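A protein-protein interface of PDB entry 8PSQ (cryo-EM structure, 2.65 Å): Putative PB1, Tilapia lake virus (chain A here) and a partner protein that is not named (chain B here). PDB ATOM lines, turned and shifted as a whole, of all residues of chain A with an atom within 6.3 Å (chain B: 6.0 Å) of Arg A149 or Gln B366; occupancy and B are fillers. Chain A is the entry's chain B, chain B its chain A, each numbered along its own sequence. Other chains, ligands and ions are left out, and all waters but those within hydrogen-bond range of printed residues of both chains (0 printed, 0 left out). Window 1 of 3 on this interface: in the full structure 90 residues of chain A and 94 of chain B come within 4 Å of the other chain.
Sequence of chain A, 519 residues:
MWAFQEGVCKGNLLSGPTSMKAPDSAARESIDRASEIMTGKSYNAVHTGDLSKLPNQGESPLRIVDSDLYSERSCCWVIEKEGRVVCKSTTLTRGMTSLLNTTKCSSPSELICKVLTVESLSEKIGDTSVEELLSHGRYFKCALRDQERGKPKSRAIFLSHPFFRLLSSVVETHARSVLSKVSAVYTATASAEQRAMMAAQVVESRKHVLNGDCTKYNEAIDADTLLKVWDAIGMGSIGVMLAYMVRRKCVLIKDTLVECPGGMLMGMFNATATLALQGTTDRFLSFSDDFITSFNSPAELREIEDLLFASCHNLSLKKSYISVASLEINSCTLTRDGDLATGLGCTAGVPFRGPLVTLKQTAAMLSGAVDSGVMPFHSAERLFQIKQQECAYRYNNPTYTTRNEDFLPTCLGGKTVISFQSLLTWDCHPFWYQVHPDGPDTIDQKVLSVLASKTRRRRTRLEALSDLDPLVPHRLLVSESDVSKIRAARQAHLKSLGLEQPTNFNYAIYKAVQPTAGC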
ATOM      1  N   TRP A   2     -22.078 -11.336   0.296  1.00  0.00           N
ATOM      2  CA  TRP A   2     -22.945 -12.487   0.078  1.00  0.00           C
ATOM      3  C   TRP A   2     -23.865 -12.740   1.263  1.00  0.00           C
ATOM      4  O   TRP A   2     -24.915 -13.367   1.095  1.00  0.00           O
ATOM      5  CB  TRP A   2     -22.108 -13.741  -0.199  1.00  0.00           C
ATOM      6  CG  TRP A   2     -20.937 -13.909   0.728  1.00  0.00           C
ATOM      7  CD1 TRP A   2     -19.642 -13.574   0.473  1.00  0.00           C
ATOM      8  CD2 TRP A   2     -20.957 -14.447   2.056  1.00  0.00           C
ATOM      9  NE1 TRP A   2     -18.854 -13.869   1.556  1.00  0.00           N
ATOM     10  CE2 TRP A   2     -19.637 -14.406   2.542  1.00  0.00           C
ATOM     11  CE3 TRP A   2     -21.963 -14.959   2.881  1.00  0.00           C
ATOM     12  CZ2 TRP A   2     -19.296 -14.856   3.814  1.00  0.00           C
ATOM     13  CZ3 TRP A   2     -21.623 -15.404   4.142  1.00  0.00           C
ATOM     14  CH2 TRP A   2     -20.301 -15.350   4.597  1.00  0.00           C
ATOM     15  N   CYS A   9     -27.702 -17.206  -2.101  1.00  0.00           N
ATOM     16  CA  CYS A   9     -26.407 -16.923  -2.705  1.00  0.00           C
ATOM     17  C   CYS A   9     -25.377 -17.887  -2.139  1.00  0.00           C
ATOM     18  O   CYS A   9     -25.266 -18.032  -0.918  1.00  0.00           O
ATOM     19  CB  CYS A   9     -25.984 -15.475  -2.443  1.00  0.00           C
ATOM     20  SG  CYS A   9     -24.511 -14.953  -3.346  1.00  0.00           S
ATOM     21  N   LYS A  10     -24.630 -18.540  -3.024  1.00  0.00           N
ATOM     22  CA  LYS A  10     -23.575 -19.462  -2.628  1.00  0.00           C
ATOM     23  C   LYS A  10     -22.201 -18.808  -2.595  1.00  0.00           C
ATOM     24  O   LYS A  10     -21.223 -19.477  -2.247  1.00  0.00           O
ATOM     25  CB  LYS A  10     -23.529 -20.673  -3.572  1.00  0.00           C
ATOM     26  CG  LYS A  10     -24.866 -21.105  -4.173  1.00  0.00           C
ATOM     27  CD  LYS A  10     -25.505 -22.236  -3.386  1.00  0.00           C
ATOM     28  CE  LYS A  10     -24.751 -23.544  -3.554  1.00  0.00           C
ATOM     29  NZ  LYS A  10     -25.558 -24.706  -3.096  1.00  0.00           N
ATOM     30  N   GLY A  11     -22.100 -17.526  -2.937  1.00  0.00           N
ATOM     31  CA  GLY A  11     -20.814 -16.861  -3.008  1.00  0.00           C
ATOM     32  C   GLY A  11     -19.913 -17.413  -4.094  1.00  0.00           C
ATOM     33  O   GLY A  11     -18.730 -17.669  -3.852  1.00  0.00           O
ATOM     34  N   ASN A  12     -20.457 -17.600  -5.295  1.00  0.00           N
ATOM     35  CA  ASN A  12     -19.723 -18.165  -6.419  1.00  0.00           C
ATOM     36  C   ASN A  12     -19.108 -17.103  -7.323  1.00  0.00           C
ATOM     37  O   ASN A  12     -18.566 -17.445  -8.376  1.00  0.00           O
ATOM     38  CB  ASN A  12     -20.642 -19.063  -7.249  1.00  0.00           C
ATOM     39  CG  ASN A  12     -20.808 -20.443  -6.656  1.00  0.00           C
ATOM     40  OD1 ASN A  12     -20.273 -20.746  -5.593  1.00  0.00           O
ATOM     41  ND2 ASN A  12     -21.555 -21.292  -7.348  1.00  0.00           N
ATOM     42  N   LEU A  13     -19.178 -15.828  -6.942  1.00  0.00           N
ATOM     43  CA  LEU A  13     -18.759 -14.769  -7.853  1.00  0.00           C
ATOM     44  C   LEU A  13     -17.252 -14.768  -8.083  1.00  0.00           C
ATOM     45  O   LEU A  13     -16.802 -14.434  -9.183  1.00  0.00           O
ATOM     46  CB  LEU A  13     -19.222 -13.411  -7.325  1.00  0.00           C
ATOM     47  CG  LEU A  13     -20.735 -13.162  -7.328  1.00  0.00           C
ATOM     48  CD1 LEU A  13     -21.025 -11.688  -7.134  1.00  0.00           C
ATOM     49  CD2 LEU A  13     -21.388 -13.656  -8.611  1.00  0.00           C
ATOM     50  N   LEU A  14     -16.463 -15.130  -7.080  1.00  0.00           N
ATOM     51  CA  LEU A  14     -15.019 -15.204  -7.244  1.00  0.00           C
ATOM     52  C   LEU A  14     -14.606 -16.615  -7.654  1.00  0.00           C
ATOM     53  O   LEU A  14     -15.378 -17.569  -7.551  1.00  0.00           O
ATOM     54  CB  LEU A  14     -14.306 -14.799  -5.955  1.00  0.00           C
ATOM     55  CG  LEU A  14     -14.614 -13.395  -5.426  1.00  0.00           C
ATOM     56  CD1 LEU A  14     -13.979 -13.192  -4.064  1.00  0.00           C
ATOM     57  CD2 LEU A  14     -14.150 -12.322  -6.394  1.00  0.00           C
ATOM     58  N   SER A  15     -13.370 -16.735  -8.130  1.00  0.00           N
ATOM     59  CA  SER A  15     -12.840 -18.033  -8.514  1.00  0.00           C
ATOM     60  C   SER A  15     -12.603 -18.899  -7.278  1.00  0.00           C
ATOM     61  O   SER A  15     -12.567 -18.420  -6.144  1.00  0.00           O
ATOM     62  CB  SER A  15     -11.537 -17.877  -9.296  1.00  0.00           C
ATOM     63  OG  SER A  15     -11.738 -17.150 -10.491  1.00  0.00           O
ATOM     64  N   GLY A  16     -12.435 -20.193  -7.515  1.00  0.00           N
ATOM     65  CA  GLY A  16     -12.201 -21.134  -6.446  1.00  0.00           C
ATOM     66  C   GLY A  16     -10.769 -21.098  -5.961  1.00  0.00           C
ATOM     67  O   GLY A  16      -9.894 -20.426  -6.524  1.00  0.00           O
ATOM     68  N   PRO A  17     -10.510 -21.837  -4.886  1.00  0.00           N
ATOM     69  CA  PRO A  17      -9.165 -21.848  -4.303  1.00  0.00           C
ATOM     70  C   PRO A  17      -8.145 -22.507  -5.215  1.00  0.00           C
ATOM     71  O   PRO A  17      -8.462 -23.401  -6.003  1.00  0.00           O
ATOM     72  CB  PRO A  17      -9.346 -22.651  -3.012  1.00  0.00           C
ATOM     73  CG  PRO A  17     -10.533 -23.505  -3.259  1.00  0.00           C
ATOM     74  CD  PRO A  17     -11.430 -22.744  -4.181  1.00  0.00           C
ATOM     75  N   GLN A 147      -9.413 -25.179  -7.451  1.00  0.00           N
ATOM     76  CA  GLN A 147     -10.484 -24.300  -7.909  1.00  0.00           C
ATOM     77  C   GLN A 147     -11.868 -24.870  -7.630  1.00  0.00           C
ATOM     78  O   GLN A 147     -12.835 -24.510  -8.305  1.00  0.00           O
ATOM     79  CB  GLN A 147     -10.340 -23.988  -9.401  1.00  0.00           C
ATOM     80  CG  GLN A 147      -9.075 -23.226  -9.740  1.00  0.00           C
ATOM     81  CD  GLN A 147      -9.301 -22.168 -10.792  1.00  0.00           C
ATOM     82  OE1 GLN A 147      -9.287 -20.972 -10.499  1.00  0.00           O
ATOM     83  NE2 GLN A 147      -9.506 -22.599 -12.030  1.00  0.00           N
ATOM     84  N   GLU A 148     -11.982 -25.755  -6.645  1.00  0.00           N
ATOM     85  CA  GLU A 148     -13.268 -26.292  -6.216  1.00  0.00           C
ATOM     86  C   GLU A 148     -13.846 -25.357  -5.162  1.00  0.00           C
ATOM     87  O   GLU A 148     -13.374 -25.329  -4.022  1.00  0.00           O
ATOM     88  CB  GLU A 148     -13.100 -27.705  -5.663  1.00  0.00           C
ATOM     89  CG  GLU A 148     -14.400 -28.462  -5.487  1.00  0.00           C
ATOM     90  CD  GLU A 148     -14.180 -29.913  -5.106  1.00  0.00           C
ATOM     91  OE1 GLU A 148     -15.141 -30.557  -4.637  1.00  0.00           O
ATOM     92  OE2 GLU A 148     -13.045 -30.408  -5.266  1.00  0.00           O
ATOM     93  N   ARG A 149     -14.868 -24.597  -5.539  1.00  0.00           N
ATOM     94  CA  ARG A 149     -15.427 -23.600  -4.636  1.00  0.00           C
ATOM     95  C   ARG A 149     -15.879 -24.246  -3.333  1.00  0.00           C
ATOM     96  O   ARG A 149     -16.527 -25.296  -3.335  1.00  0.00           O
ATOM     97  CB  ARG A 149     -16.598 -22.886  -5.304  1.00  0.00           C
ATOM     98  CG  ARG A 149     -16.232 -21.551  -5.920  1.00  0.00           C
ATOM     99  CD  ARG A 149     -17.204 -21.143  -7.006  1.00  0.00           C
ATOM    100  NE  ARG A 149     -16.572 -20.292  -8.008  1.00  0.00           N
ATOM    101  CZ  ARG A 149     -16.778 -20.376  -9.315  1.00  0.00           C
ATOM    102  NH1 ARG A 149     -17.600 -21.273  -9.833  1.00  0.00           N
ATOM    103  NH2 ARG A 149     -16.147 -19.533 -10.124  1.00  0.00           N
ATOM    104  N   GLY A 150     -15.532 -23.610  -2.216  1.00  0.00           N
ATOM    105  CA  GLY A 150     -15.929 -24.091  -0.911  1.00  0.00           C
ATOM    106  C   GLY A 150     -15.018 -25.128  -0.296  1.00  0.00           C
ATOM    107  O   GLY A 150     -15.378 -25.705   0.735  1.00  0.00           O
ATOM    108  N   LYS A 151     -13.852 -25.386  -0.886  1.00  0.00           N
ATOM    109  CA  LYS A 151     -12.898 -26.367  -0.370  1.00  0.00           C
ATOM    110  C   LYS A 151     -11.528 -25.709  -0.272  1.00  0.00           C
ATOM    111  O   LYS A 151     -10.680 -25.878  -1.158  1.00  0.00           O
ATOM    112  CB  LYS A 151     -12.849 -27.612  -1.257  1.00  0.00           C
ATOM    113  CG  LYS A 151     -14.154 -28.394  -1.310  1.00  0.00           C
ATOM    114  CD  LYS A 151     -14.537 -28.993   0.041  1.00  0.00           C
ATOM    115  CE  LYS A 151     -13.600 -30.116   0.451  1.00  0.00           C
ATOM    116  NZ  LYS A 151     -14.019 -30.766   1.724  1.00  0.00           N
ATOM    117  N   PRO A 152     -11.275 -24.949   0.798  1.00  0.00           N
ATOM    118  CA  PRO A 152      -9.964 -24.291   0.930  1.00  0.00           C
ATOM    119  C   PRO A 152      -8.797 -25.261   0.880  1.00  0.00           C
ATOM    120  O   PRO A 152      -7.743 -24.926   0.327  1.00  0.00           O
ATOM    121  CB  PRO A 152     -10.065 -23.591   2.292  1.00  0.00           C
ATOM    122  CG  PRO A 152     -11.520 -23.411   2.517  1.00  0.00           C
ATOM    123  CD  PRO A 152     -12.181 -24.598   1.902  1.00  0.00           C
ATOM    124  N   LYS A 319     -23.408 -31.040   6.771  1.00  0.00           N
ATOM    125  CA  LYS A 319     -24.063 -30.311   5.692  1.00  0.00           C
ATOM    126  C   LYS A 319     -25.527 -30.668   5.493  1.00  0.00           C
ATOM    127  O   LYS A 319     -26.316 -29.786   5.153  1.00  0.00           O
ATOM    128  CB  LYS A 319     -23.325 -30.547   4.370  1.00  0.00           C
ATOM    129  CG  LYS A 319     -21.867 -30.128   4.388  1.00  0.00           C
ATOM    130  CD  LYS A 319     -21.172 -30.513   3.097  1.00  0.00           C
ATOM    131  CE  LYS A 319     -19.702 -30.141   3.123  1.00  0.00           C
ATOM    132  NZ  LYS A 319     -19.465 -28.749   2.653  1.00  0.00           N
ATOM    133  N   CYS A 346     -26.366 -19.905  -7.944  1.00  0.00           N
ATOM    134  CA  CYS A 346     -25.059 -20.414  -8.332  1.00  0.00           C
ATOM    135  C   CYS A 346     -24.348 -19.524  -9.338  1.00  0.00           C
ATOM    136  O   CYS A 346     -23.310 -19.927  -9.868  1.00  0.00           O
ATOM    137  CB  CYS A 346     -25.194 -21.823  -8.911  1.00  0.00           C
ATOM    138  SG  CYS A 346     -26.066 -22.964  -7.841  1.00  0.00           S
ATOM    139  N   ALA A 348     -21.928 -17.547 -11.249  1.00  0.00           N
ATOM    140  CA  ALA A 348     -20.481 -17.519 -11.104  1.00  0.00           C
ATOM    141  C   ALA A 348     -19.902 -16.364 -11.906  1.00  0.00           C
ATOM    142  O   ALA A 348     -20.349 -16.086 -13.023  1.00  0.00           O
ATOM    143  CB  ALA A 348     -19.859 -18.838 -11.564  1.00  0.00           C
ATOM    144  N   GLY A 349     -18.913 -15.692 -11.329  1.00  0.00           N
ATOM    145  CA  GLY A 349     -18.231 -14.635 -12.040  1.00  0.00           C
ATOM    146  C   GLY A 349     -17.276 -15.174 -13.084  1.00  0.00           C
ATOM    147  O   GLY A 349     -16.896 -16.344 -13.087  1.00  0.00           O
ATOM    148  N   PRO A 351     -13.569 -14.723 -14.564  1.00  0.00           N
ATOM    149  CA  PRO A 351     -12.254 -14.105 -14.366  1.00  0.00           C
ATOM    150  C   PRO A 351     -11.688 -13.584 -15.677  1.00  0.00           C
ATOM    151  O   PRO A 351     -12.200 -13.849 -16.765  1.00  0.00           O
ATOM    152  CB  PRO A 351     -11.407 -15.246 -13.802  1.00  0.00           C
ATOM    153  CG  PRO A 351     -12.039 -16.473 -14.336  1.00  0.00           C
ATOM    154  CD  PRO A 351     -13.509 -16.189 -14.427  1.00  0.00           C
ATOM    155  N   SER B 361     -13.893 -17.719   2.399  1.00  0.00           N
ATOM    156  CA  SER B 361     -15.168 -17.017   2.438  1.00  0.00           C
ATOM    157  C   SER B 361     -16.231 -17.751   1.634  1.00  0.00           C
ATOM    158  O   SER B 361     -17.415 -17.668   1.960  1.00  0.00           O
ATOM    159  CB  SER B 361     -14.995 -15.591   1.918  1.00  0.00           C
ATOM    160  OG  SER B 361     -15.058 -15.550   0.504  1.00  0.00           O
ATOM    161  N   GLN B 362     -15.833 -18.485   0.593  1.00  0.00           N
ATOM    162  CA  GLN B 362     -16.805 -19.252  -0.180  1.00  0.00           C
ATOM    163  C   GLN B 362     -17.373 -20.410   0.632  1.00  0.00           C
ATOM    164  O   GLN B 362     -18.574 -20.695   0.564  1.00  0.00           O
ATOM    165  CB  GLN B 362     -16.163 -19.760  -1.468  1.00  0.00           C
ATOM    166  CG  GLN B 362     -15.798 -18.658  -2.444  1.00  0.00           C
ATOM    167  CD  GLN B 362     -15.044 -19.173  -3.650  1.00  0.00           C
ATOM    168  OE1 GLN B 362     -14.497 -20.272  -3.629  1.00  0.00           O
ATOM    169  NE2 GLN B 362     -15.019 -18.383  -4.712  1.00  0.00           N
ATOM    170  N   ALA B 363     -16.525 -21.094   1.402  1.00  0.00           N
ATOM    171  CA  ALA B 363     -17.022 -22.140   2.290  1.00  0.00           C
ATOM    172  C   ALA B 363     -17.965 -21.561   3.335  1.00  0.00           C
ATOM    173  O   ALA B 363     -19.030 -22.133   3.613  1.00  0.00           O
ATOM    174  CB  ALA B 363     -15.852 -22.856   2.961  1.00  0.00           C
ATOM    175  N   VAL B 364     -17.599 -20.416   3.916  1.00  0.00           N
ATOM    176  CA  VAL B 364     -18.476 -19.786   4.899  1.00  0.00           C
ATOM    177  C   VAL B 364     -19.800 -19.392   4.252  1.00  0.00           C
ATOM    178  O   VAL B 364     -20.866 -19.532   4.858  1.00  0.00           O
ATOM    179  CB  VAL B 364     -17.780 -18.578   5.551  1.00  0.00           C
ATOM    180  CG1 VAL B 364     -18.685 -17.938   6.589  1.00  0.00           C
ATOM    181  CG2 VAL B 364     -16.473 -19.002   6.190  1.00  0.00           C
ATOM    182  N   ALA B 365     -19.753 -18.891   3.017  1.00  0.00           N
ATOM    183  CA  ALA B 365     -20.970 -18.484   2.325  1.00  0.00           C
ATOM    184  C   ALA B 365     -21.875 -19.674   2.038  1.00  0.00           C
ATOM    185  O   ALA B 365     -23.097 -19.581   2.189  1.00  0.00           O
ATOM    186  CB  ALA B 365     -20.614 -17.762   1.026  1.00  0.00           C
ATOM    187  N   GLN B 366     -21.298 -20.797   1.608  1.00  0.00           N
ATOM    188  CA  GLN B 366     -22.108 -21.984   1.356  1.00  0.00           C
ATOM    189  C   GLN B 366     -22.754 -22.489   2.641  1.00  0.00           C
ATOM    190  O   GLN B 366     -23.942 -22.847   2.655  1.00  0.00           O
ATOM    191  CB  GLN B 366     -21.251 -23.075   0.717  1.00  0.00           C
ATOM    192  CG  GLN B 366     -20.958 -22.832  -0.752  1.00  0.00           C
ATOM    193  CD  GLN B 366     -20.031 -23.872  -1.343  1.00  0.00           C
ATOM    194  OE1 GLN B 366     -19.829 -24.938  -0.767  1.00  0.00           O
ATOM    195  NE2 GLN B 366     -19.458 -23.563  -2.498  1.00  0.00           N
ATOM    196  N   HIS B 367     -21.996 -22.514   3.740  1.00  0.00           N
ATOM    197  CA  HIS B 367     -22.582 -22.963   4.997  1.00  0.00           C
ATOM    198  C   HIS B 367     -23.654 -21.995   5.485  1.00  0.00           C
ATOM    199  O   HIS B 367     -24.656 -22.415   6.069  1.00  0.00           O
ATOM    200  CB  HIS B 367     -21.506 -23.147   6.062  1.00  0.00           C
ATOM    201  CG  HIS B 367     -21.887 -24.126   7.127  1.00  0.00           C
ATOM    202  ND1 HIS B 367     -22.181 -25.443   6.852  1.00  0.00           N
ATOM    203  CD2 HIS B 367     -22.046 -23.976   8.463  1.00  0.00           C
ATOM    204  CE1 HIS B 367     -22.492 -26.066   7.975  1.00  0.00           C
ATOM    205  NE2 HIS B 367     -22.417 -25.198   8.966  1.00  0.00           N
ATOM    206  N   PHE B 368     -23.467 -20.695   5.256  1.00  0.00           N
ATOM    207  CA  PHE B 368     -24.483 -19.728   5.659  1.00  0.00           C
ATOM    208  C   PHE B 368     -25.743 -19.869   4.812  1.00  0.00           C
ATOM    209  O   PHE B 368     -26.855 -19.671   5.309  1.00  0.00           O
ATOM    210  CB  PHE B 368     -23.927 -18.310   5.562  1.00  0.00           C
ATOM    211  CG  PHE B 368     -24.844 -17.261   6.121  1.00  0.00           C
ATOM    212  CD1 PHE B 368     -25.357 -17.378   7.401  1.00  0.00           C
ATOM    213  CD2 PHE B 368     -25.198 -16.159   5.365  1.00  0.00           C
ATOM    214  CE1 PHE B 368     -26.200 -16.420   7.914  1.00  0.00           C
ATOM    215  CE2 PHE B 368     -26.040 -15.196   5.875  1.00  0.00           C
ATOM    216  CZ  PHE B 368     -26.540 -15.326   7.152  1.00  0.00           C
ATOM    217  N   ASN B 369     -25.589 -20.199   3.531  1.00  0.00           N
ATOM    218  CA  ASN B 369     -26.754 -20.500   2.706  1.00  0.00           C
ATOM    219  C   ASN B 369     -27.507 -21.705   3.254  1.00  0.00           C
ATOM    220  O   ASN B 369     -28.742 -21.686   3.359  1.00  0.00           O
ATOM    221  CB  ASN B 369     -26.317 -20.744   1.263  1.00  0.00           C
ATOM    222  CG  ASN B 369     -27.452 -20.596   0.279  1.00  0.00           C
ATOM    223  OD1 ASN B 369     -28.079 -19.541   0.192  1.00  0.00           O
ATOM    224  ND2 ASN B 369     -27.718 -21.650  -0.479  1.00  0.00           N
ATOM    225  N   ARG B 370     -26.776 -22.758   3.626  1.00  0.00           N
ATOM    226  CA  ARG B 370     -27.413 -23.909   4.260  1.00  0.00           C
ATOM    227  C   ARG B 370     -28.139 -23.496   5.534  1.00  0.00           C
ATOM    228  O   ARG B 370     -29.260 -23.944   5.798  1.00  0.00           O
ATOM    229  CB  ARG B 370     -26.369 -24.980   4.571  1.00  0.00           C
ATOM    230  CG  ARG B 370     -26.031 -25.887   3.410  1.00  0.00           C
ATOM    231  CD  ARG B 370     -25.161 -27.044   3.862  1.00  0.00           C
ATOM    232  NE  ARG B 370     -23.762 -26.659   4.005  1.00  0.00           N
ATOM    233  CZ  ARG B 370     -22.868 -26.682   3.028  1.00  0.00           C
ATOM    234  NH1 ARG B 370     -23.185 -27.075   1.806  1.00  0.00           N
ATOM    235  NH2 ARG B 370     -21.620 -26.302   3.283  1.00  0.00           N
ATOM    236  N   HIS B 371     -27.506 -22.639   6.335  1.00  0.00           N
ATOM    237  CA  HIS B 371     -28.110 -22.139   7.565  1.00  0.00           C
ATOM    238  C   HIS B 371     -29.421 -21.418   7.278  1.00  0.00           C
ATOM    239  O   HIS B 371     -30.421 -21.615   7.975  1.00  0.00           O
ATOM    240  CB  HIS B 371     -27.111 -21.208   8.258  1.00  0.00           C
ATOM    241  CG  HIS B 371     -27.506 -20.775   9.638  1.00  0.00           C
ATOM    242  ND1 HIS B 371     -28.816 -20.659  10.050  1.00  0.00           N
ATOM    243  CD2 HIS B 371     -26.748 -20.399  10.694  1.00  0.00           C
ATOM    244  CE1 HIS B 371     -28.846 -20.244  11.303  1.00  0.00           C
ATOM    245  NE2 HIS B 371     -27.604 -20.080  11.718  1.00  0.00           N
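Of the 21 printed residues of chain A, 11 touch a printed residue of chain B. Printed residues of chain A that touch a printed residue of chain B: Trp A2, Cys A9, Lys A10, Gly A11, Leu A14, Ser A15, Gly A16, Pro A17, Arg A149, Gly A150 and Lys A319. Hydrophobic or aromatic side chains of chain A that line the printed part of chain B: Trp A2, Leu A14 and Pro A17. Of the 11 printed residues of chain B, 9 touch a printed residue of chain A. Hydrophobic or aromatic side chains of chain B that line the printed part of chain A: Ala B363, Val B364, Ala B365 and Phe B368.
A ring nitrogen (ND1) of His B367 sits at hydrogen-bond distance from the guanidinium group (NE) of Arg B370. The side-chain sulfur (SG) of Cys A9 sits close to the backbone NH (N) of Gly A11. O of Asn A12 lies within hydrogen-bond range of NE of Arg A149 (3.5 Å). The backbone NH (N) of Gln A147 sits at hydrogen-bond distance from the backbone carbonyl oxygen (O) of Pro A17 (2.5 Å). The guanidinium group (NE) of Arg A149 sits at hydrogen-bond distance from the backbone carbonyl oxygen (O) of Leu A14 (3.0 Å).
The side-chain amide nitrogen of Gln B362 is in hydrogen-bond range of the backbone carbonyl oxygen of Ser A15 (2.8 Å). The guanidinium group (NH2) of Arg B370 lies close to the side-chain amino group (NZ) of Lys A319, 3.3 Å away. The backbone NH (N) of Cys A9 sits at hydrogen-bond distance from the side-chain amide oxygen (OD1) of Asn B369 (3.3 Å). The backbone carbonyl oxygen (O) of Leu A14 sits at hydrogen-bond distance from the side-chain amide nitrogen (NE2) of Gln B362, at 3.0 Å.
Of the printed residues of chain B, Cys A9 touches Asn B369 (3.3 Å). Of the printed residues of chain B, Lys A10 touches Ala B365, Gln B366 and Asn B369. Of the printed residues of chain B, Leu A14 touches Gln B362. Of the printed residues of chain B, Ser A15 touches Gln B362. Printed residues of chain B within 4 Å of Pro A17: Gln B362 (3.98 Å). Gln B366 touches just these residues of chain A: Lys A10 (3.7 Å), Arg A149 (3.5 Å) and Gly A150 (3.9 Å). His B367 touches none of the printed residues of chain A. The nearest residue of chain B that does not touch Arg A149 is Ala B363 (5.7 Å). The nearest printed residue of chain B that does not touch Gly A11 is Ala B365 (4.1 Å).
Among the printed residues, merely in contact across the chains: Trp A2 with Ser B361 (3.9 Å), Trp A2 with Val B364 (3.6 Å), Trp A2 with Ala B365 (3.5 Å), Trp A2 with Phe B368 (3.9 Å), Lys A10 with Ala B365 (3.7 Å), Lys A10 with Gln B366 (3.7 Å), Lys A10 with Asn B369 (3.7 Å), Gly A11 with Gln B362 (3.4 Å), Gly A16 with Gln B362 (3.7 Å), Pro A17 with Gln B362 (3.98 Å), Arg A149 with Gln B362 (3.1 Å), Arg A149 with Gln B366 (3.5 Å), Gly A150 with Gln B362 (3.8 Å), Gly A150 with Ala B363 (3.6 Å) and Gly A150 with Gln B366 (3.9 Å).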
